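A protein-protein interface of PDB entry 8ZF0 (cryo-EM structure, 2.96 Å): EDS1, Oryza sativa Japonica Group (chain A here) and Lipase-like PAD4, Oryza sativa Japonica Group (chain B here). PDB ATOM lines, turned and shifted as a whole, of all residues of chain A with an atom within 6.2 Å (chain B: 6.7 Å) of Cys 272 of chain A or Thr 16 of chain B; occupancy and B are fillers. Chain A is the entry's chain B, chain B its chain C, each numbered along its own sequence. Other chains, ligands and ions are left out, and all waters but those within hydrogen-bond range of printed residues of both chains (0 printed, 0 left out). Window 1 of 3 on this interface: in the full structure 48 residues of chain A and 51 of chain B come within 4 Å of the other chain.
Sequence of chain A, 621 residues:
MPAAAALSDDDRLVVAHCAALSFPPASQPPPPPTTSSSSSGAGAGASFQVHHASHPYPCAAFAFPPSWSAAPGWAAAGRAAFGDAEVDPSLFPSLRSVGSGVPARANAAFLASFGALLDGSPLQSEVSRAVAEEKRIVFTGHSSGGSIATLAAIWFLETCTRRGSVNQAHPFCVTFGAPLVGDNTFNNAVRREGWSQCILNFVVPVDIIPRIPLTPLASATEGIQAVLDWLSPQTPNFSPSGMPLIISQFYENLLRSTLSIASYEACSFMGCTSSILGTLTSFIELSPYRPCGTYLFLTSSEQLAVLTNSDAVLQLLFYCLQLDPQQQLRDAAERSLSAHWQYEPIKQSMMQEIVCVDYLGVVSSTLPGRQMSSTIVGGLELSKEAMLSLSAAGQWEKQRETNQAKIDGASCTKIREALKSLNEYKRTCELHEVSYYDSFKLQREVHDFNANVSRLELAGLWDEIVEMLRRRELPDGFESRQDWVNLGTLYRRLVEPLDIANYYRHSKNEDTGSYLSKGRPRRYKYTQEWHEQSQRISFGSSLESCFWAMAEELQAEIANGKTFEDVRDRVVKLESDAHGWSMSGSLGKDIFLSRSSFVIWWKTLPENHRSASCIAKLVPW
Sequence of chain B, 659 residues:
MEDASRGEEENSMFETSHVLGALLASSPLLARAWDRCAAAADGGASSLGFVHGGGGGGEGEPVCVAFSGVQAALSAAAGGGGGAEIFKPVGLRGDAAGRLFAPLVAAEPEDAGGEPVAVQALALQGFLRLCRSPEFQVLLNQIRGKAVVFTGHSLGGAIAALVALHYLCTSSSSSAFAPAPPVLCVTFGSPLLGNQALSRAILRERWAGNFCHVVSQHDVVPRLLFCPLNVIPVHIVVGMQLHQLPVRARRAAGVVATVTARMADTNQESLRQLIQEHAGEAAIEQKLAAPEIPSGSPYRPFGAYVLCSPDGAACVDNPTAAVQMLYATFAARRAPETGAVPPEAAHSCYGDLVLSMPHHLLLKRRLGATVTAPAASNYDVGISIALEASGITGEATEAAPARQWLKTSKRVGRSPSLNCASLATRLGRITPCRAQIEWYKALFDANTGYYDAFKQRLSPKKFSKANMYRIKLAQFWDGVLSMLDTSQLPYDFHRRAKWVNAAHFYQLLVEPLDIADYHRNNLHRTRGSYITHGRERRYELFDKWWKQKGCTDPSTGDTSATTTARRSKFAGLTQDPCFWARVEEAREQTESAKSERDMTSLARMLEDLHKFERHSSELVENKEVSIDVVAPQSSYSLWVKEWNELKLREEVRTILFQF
The backbone NH (N) of Cys 272 of chain A is in hydrogen-bond range of the backbone carbonyl oxygen (O) of Cys 267 of chain A (3.5 Å). NZ of Lys 410 of chain B lies within hydrogen-bond range of O of Phe 14 of chain B (2.7 Å). The side-chain carboxylate (OE2) of Glu 15 of chain B sits at hydrogen-bond distance from the side-chain hydroxyl (OG) of Ser 17 of chain B (2.7 Å).
Among the printed residues, merely in contact across the chains: Cys 267 of chain A with Val 19 of chain B, Met 270 of chain A with Phe 14 of chain B, Met 270 of chain A with Glu 15 of chain B, Cys 272 of chain A with Thr 16 of chain B and Leu 277 of chain A with Leu 20 of chain B.
Cys 272 of chain A touches just one residue of chain B: Thr 16. Of chain A, only Cys 272 comes within 4 Å of Thr 16 of chain B. Of the printed residues of chain B, Leu 277 of chain A touches Leu 20 (3.97 Å). Of the printed residues of chain B, Cys 267 of chain A touches Val 19 (3.7 Å). Printed residues of chain A within 4 Å of Glu 15 of chain B: Met 270 (3.98 Å). Of the printed residues of chain B, Met 270 of chain A touches Phe 14 and Glu 15. Printed residues of chain A within 4 Å of Val 19 of chain B: Cys 267. The nearest residue of chain B that does not touch Cys 272 of chain A is Lys 410 of chain B (5.8 Å).
Of the 8 printed residues of chain A, 4 touch a printed residue of chain B. Among the printed residues, no Asp or Glu carboxylate lies within 4 Å of a Lys or Arg side-chain nitrogen of the other chain.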
ATOM      1  N   CYS A 267      26.320 -32.232  25.731  1.00  0.00           N
ATOM      2  CA  CYS A 267      24.891 -32.002  25.912  1.00  0.00           C
ATOM      3  C   CYS A 267      24.079 -33.273  25.699  1.00  0.00           C
ATOM      4  O   CYS A 267      22.926 -33.350  26.140  1.00  0.00           O
ATOM      5  CB  CYS A 267      24.414 -30.904  24.962  1.00  0.00           C
ATOM      6  SG  CYS A 267      25.216 -29.304  25.204  1.00  0.00           S
ATOM      7  N   SER A 268      24.652 -34.272  25.025  1.00  0.00           N
ATOM      8  CA  SER A 268      23.916 -35.503  24.758  1.00  0.00           C
ATOM      9  C   SER A 268      23.668 -36.291  26.040  1.00  0.00           C
ATOM     10  O   SER A 268      22.545 -36.738  26.297  1.00  0.00           O
ATOM     11  CB  SER A 268      24.673 -36.355  23.738  1.00  0.00           C
ATOM     12  OG  SER A 268      24.871 -35.645  22.528  1.00  0.00           O
ATOM     13  N   MET A 270      24.166 -35.076  29.154  1.00  0.00           N
ATOM     14  CA  MET A 270      23.890 -34.196  30.280  1.00  0.00           C
ATOM     15  C   MET A 270      22.424 -33.815  30.413  1.00  0.00           C
ATOM     16  O   MET A 270      21.997 -33.458  31.515  1.00  0.00           O
ATOM     17  CB  MET A 270      24.728 -32.912  30.176  1.00  0.00           C
ATOM     18  CG  MET A 270      25.525 -32.592  31.429  1.00  0.00           C
ATOM     19  SD  MET A 270      26.600 -31.158  31.230  1.00  0.00           S
ATOM     20  CE  MET A 270      28.214 -31.929  31.337  1.00  0.00           C
ATOM     21  N   GLY A 271      21.651 -33.880  29.333  1.00  0.00           N
ATOM     22  CA  GLY A 271      20.231 -33.598  29.407  1.00  0.00           C
ATOM     23  C   GLY A 271      19.859 -32.190  28.994  1.00  0.00           C
ATOM     24  O   GLY A 271      18.971 -31.577  29.596  1.00  0.00           O
ATOM     25  N   CYS A 272      20.530 -31.660  27.971  1.00  0.00           N
ATOM     26  CA  CYS A 272      20.209 -30.320  27.490  1.00  0.00           C
ATOM     27  C   CYS A 272      18.866 -30.309  26.769  1.00  0.00           C
ATOM     28  O   CYS A 272      17.924 -29.630  27.194  1.00  0.00           O
ATOM     29  CB  CYS A 272      21.322 -29.810  26.574  1.00  0.00           C
ATOM     30  N   THR A 273      18.762 -31.066  25.677  1.00  0.00           N
ATOM     31  CA  THR A 273      17.530 -31.205  24.899  1.00  0.00           C
ATOM     32  C   THR A 273      16.981 -29.835  24.493  1.00  0.00           C
ATOM     33  O   THR A 273      15.899 -29.413  24.903  1.00  0.00           O
ATOM     34  CB  THR A 273      16.485 -32.017  25.671  1.00  0.00           C
ATOM     35  OG1 THR A 273      17.116 -33.155  26.271  1.00  0.00           O
ATOM     36  CG2 THR A 273      15.388 -32.504  24.733  1.00  0.00           C
ATOM     37  N   SER A 274      17.765 -29.135  23.680  1.00  0.00           N
ATOM     38  CA  SER A 274      17.405 -27.811  23.196  1.00  0.00           C
ATOM     39  C   SER A 274      17.020 -27.871  21.723  1.00  0.00           C
ATOM     40  O   SER A 274      17.623 -28.603  20.933  1.00  0.00           O
ATOM     41  CB  SER A 274      18.558 -26.825  23.394  1.00  0.00           C
ATOM     42  N   LEU A 277      19.851 -27.065  19.164  1.00  0.00           N
ATOM     43  CA  LEU A 277      20.954 -27.991  18.924  1.00  0.00           C
ATOM     44  C   LEU A 277      20.821 -28.679  17.572  1.00  0.00           C
ATOM     45  O   LEU A 277      21.817 -28.859  16.861  1.00  0.00           O
ATOM     46  CB  LEU A 277      21.021 -29.026  20.048  1.00  0.00           C
ATOM     47  CG  LEU A 277      22.204 -28.914  21.011  1.00  0.00           C
ATOM     48  CD1 LEU A 277      22.367 -30.197  21.811  1.00  0.00           C
ATOM     49  CD2 LEU A 277      23.484 -28.581  20.259  1.00  0.00           C
ATOM     50  N   PHE B  14      22.516 -31.283  36.107  1.00  0.00           N
ATOM     51  CA  PHE B  14      23.679 -30.519  35.684  1.00  0.00           C
ATOM     52  C   PHE B  14      23.247 -29.308  34.868  1.00  0.00           C
ATOM     53  O   PHE B  14      22.213 -29.327  34.193  1.00  0.00           O
ATOM     54  CB  PHE B  14      24.644 -31.380  34.857  1.00  0.00           C
ATOM     55  CG  PHE B  14      25.301 -32.481  35.640  1.00  0.00           C
ATOM     56  CD1 PHE B  14      24.622 -33.657  35.913  1.00  0.00           C
ATOM     57  CD2 PHE B  14      26.598 -32.340  36.104  1.00  0.00           C
ATOM     58  CE1 PHE B  14      25.224 -34.670  36.633  1.00  0.00           C
ATOM     59  CE2 PHE B  14      27.206 -33.349  36.825  1.00  0.00           C
ATOM     60  CZ  PHE B  14      26.518 -34.516  37.090  1.00  0.00           C
ATOM     61  N   GLU B  15      24.054 -28.253  34.938  1.00  0.00           N
ATOM     62  CA  GLU B  15      23.805 -27.030  34.189  1.00  0.00           C
ATOM     63  C   GLU B  15      24.436 -27.148  32.807  1.00  0.00           C
ATOM     64  O   GLU B  15      25.577 -27.596  32.671  1.00  0.00           O
ATOM     65  CB  GLU B  15      24.376 -25.825  34.939  1.00  0.00           C
ATOM     66  CG  GLU B  15      24.440 -24.538  34.136  1.00  0.00           C
ATOM     67  CD  GLU B  15      23.069 -23.933  33.896  1.00  0.00           C
ATOM     68  OE1 GLU B  15      22.094 -24.379  34.537  1.00  0.00           O
ATOM     69  OE2 GLU B  15      22.968 -23.001  33.074  1.00  0.00           O
ATOM     70  N   THR B  16      23.682 -26.753  31.777  1.00  0.00           N
ATOM     71  CA  THR B  16      24.102 -26.960  30.398  1.00  0.00           C
ATOM     72  C   THR B  16      24.225 -25.688  29.570  1.00  0.00           C
ATOM     73  O   THR B  16      24.606 -25.778  28.398  1.00  0.00           O
ATOM     74  CB  THR B  16      23.132 -27.913  29.678  1.00  0.00           C
ATOM     75  OG1 THR B  16      21.927 -27.213  29.350  1.00  0.00           O
ATOM     76  CG2 THR B  16      22.797 -29.110  30.555  1.00  0.00           C
ATOM     77  N   SER B  17      23.910 -24.516  30.127  1.00  0.00           N
ATOM     78  CA  SER B  17      23.947 -23.293  29.329  1.00  0.00           C
ATOM     79  C   SER B  17      25.369 -22.936  28.908  1.00  0.00           C
ATOM     80  O   SER B  17      25.595 -22.521  27.765  1.00  0.00           O
ATOM     81  CB  SER B  17      23.315 -22.138  30.103  1.00  0.00           C
ATOM     82  OG  SER B  17      24.207 -21.629  31.078  1.00  0.00           O
ATOM     83  N   HIS B  18      26.338 -23.084  29.815  1.00  0.00           N
ATOM     84  CA  HIS B  18      27.708 -22.709  29.483  1.00  0.00           C
ATOM     85  C   HIS B  18      28.304 -23.622  28.420  1.00  0.00           C
ATOM     86  O   HIS B  18      29.115 -23.171  27.605  1.00  0.00           O
ATOM     87  CB  HIS B  18      28.585 -22.708  30.737  1.00  0.00           C
ATOM     88  CG  HIS B  18      28.517 -23.975  31.529  1.00  0.00           C
ATOM     89  ND1 HIS B  18      27.452 -24.289  32.347  1.00  0.00           N
ATOM     90  CD2 HIS B  18      29.387 -25.008  31.633  1.00  0.00           C
ATOM     91  CE1 HIS B  18      27.668 -25.459  32.918  1.00  0.00           C
ATOM     92  NE2 HIS B  18      28.835 -25.918  32.502  1.00  0.00           N
ATOM     93  N   VAL B  19      27.916 -24.899  28.406  1.00  0.00           N
ATOM     94  CA  VAL B  19      28.398 -25.810  27.370  1.00  0.00           C
ATOM     95  C   VAL B  19      27.906 -25.360  26.000  1.00  0.00           C
ATOM     96  O   VAL B  19      28.666 -25.328  25.023  1.00  0.00           O
ATOM     97  CB  VAL B  19      27.965 -27.253  27.681  1.00  0.00           C
ATOM     98  CG1 VAL B  19      28.437 -28.196  26.587  1.00  0.00           C
ATOM     99  CG2 VAL B  19      28.500 -27.688  29.036  1.00  0.00           C
ATOM    100  N   LEU B  20      26.625 -24.997  25.909  1.00  0.00           N
ATOM    101  CA  LEU B  20      26.079 -24.508  24.646  1.00  0.00           C
ATOM    102  C   LEU B  20      26.725 -23.189  24.240  1.00  0.00           C
ATOM    103  O   LEU B  20      26.989 -22.959  23.053  1.00  0.00           O
ATOM    104  CB  LEU B  20      24.562 -24.357  24.755  1.00  0.00           C
ATOM    105  CG  LEU B  20      23.802 -24.196  23.439  1.00  0.00           C
ATOM    106  CD1 LEU B  20      24.090 -25.363  22.510  1.00  0.00           C
ATOM    107  CD2 LEU B  20      22.309 -24.074  23.699  1.00  0.00           C
ATOM    108  N   GLY B  21      26.983 -22.308  25.209  1.00  0.00           N
ATOM    109  CA  GLY B  21      27.673 -21.067  24.896  1.00  0.00           C
ATOM    110  C   GLY B  21      29.076 -21.297  24.367  1.00  0.00           C
ATOM    111  O   GLY B  21      29.511 -20.634  23.423  1.00  0.00           O
ATOM    112  N   CYS B 315      23.843 -19.412  27.102  1.00  0.00           N
ATOM    113  CA  CYS B 315      22.685 -19.471  26.221  1.00  0.00           C
ATOM    114  C   CYS B 315      21.439 -19.785  27.040  1.00  0.00           C
ATOM    115  O   CYS B 315      21.413 -20.772  27.782  1.00  0.00           O
ATOM    116  CB  CYS B 315      22.885 -20.522  25.130  1.00  0.00           C
ATOM    117  SG  CYS B 315      21.635 -20.495  23.828  1.00  0.00           S
ATOM    118  N   TYR B 379      25.134 -29.095  40.492  1.00  0.00           N
ATOM    119  CA  TYR B 379      24.243 -28.117  39.878  1.00  0.00           C
ATOM    120  C   TYR B 379      24.611 -26.700  40.299  1.00  0.00           C
ATOM    121  O   TYR B 379      24.603 -25.776  39.476  1.00  0.00           O
ATOM    122  CB  TYR B 379      22.792 -28.432  40.245  1.00  0.00           C
ATOM    123  CG  TYR B 379      21.769 -27.620  39.485  1.00  0.00           C
ATOM    124  CD1 TYR B 379      21.780 -27.577  38.096  1.00  0.00           C
ATOM    125  CD2 TYR B 379      20.787 -26.903  40.154  1.00  0.00           C
ATOM    126  CE1 TYR B 379      20.845 -26.838  37.397  1.00  0.00           C
ATOM    127  CE2 TYR B 379      19.847 -26.162  39.463  1.00  0.00           C
ATOM    128  CZ  TYR B 379      19.881 -26.133  38.085  1.00  0.00           C
ATOM    129  OH  TYR B 379      18.948 -25.396  37.394  1.00  0.00           O
ATOM    130  N   GLY B 382      27.734 -25.700  38.404  1.00  0.00           N
ATOM    131  CA  GLY B 382      27.403 -25.322  37.040  1.00  0.00           C
ATOM    132  C   GLY B 382      26.739 -23.961  36.956  1.00  0.00           C
ATOM    133  O   GLY B 382      27.033 -23.170  36.057  1.00  0.00           O
ATOM    134  N   LYS B 410      15.149 -24.407  34.710  1.00  0.00           N
ATOM    135  CA  LYS B 410      15.325 -25.840  34.524  1.00  0.00           C
ATOM    136  C   LYS B 410      14.081 -26.602  34.964  1.00  0.00           C
ATOM    137  O   LYS B 410      13.482 -26.306  36.001  1.00  0.00           O
ATOM    138  CB  LYS B 410      16.544 -26.330  35.304  1.00  0.00           C
ATOM    139  CG  LYS B 410      16.970 -27.749  34.964  1.00  0.00           C
ATOM    140  CD  LYS B 410      18.172 -27.756  34.034  1.00  0.00           C
ATOM    141  CE  LYS B 410      18.308 -29.088  33.316  1.00  0.00           C
ATOM    142  NZ  LYS B 410      19.721 -29.554  33.270  1.00  0.00           N
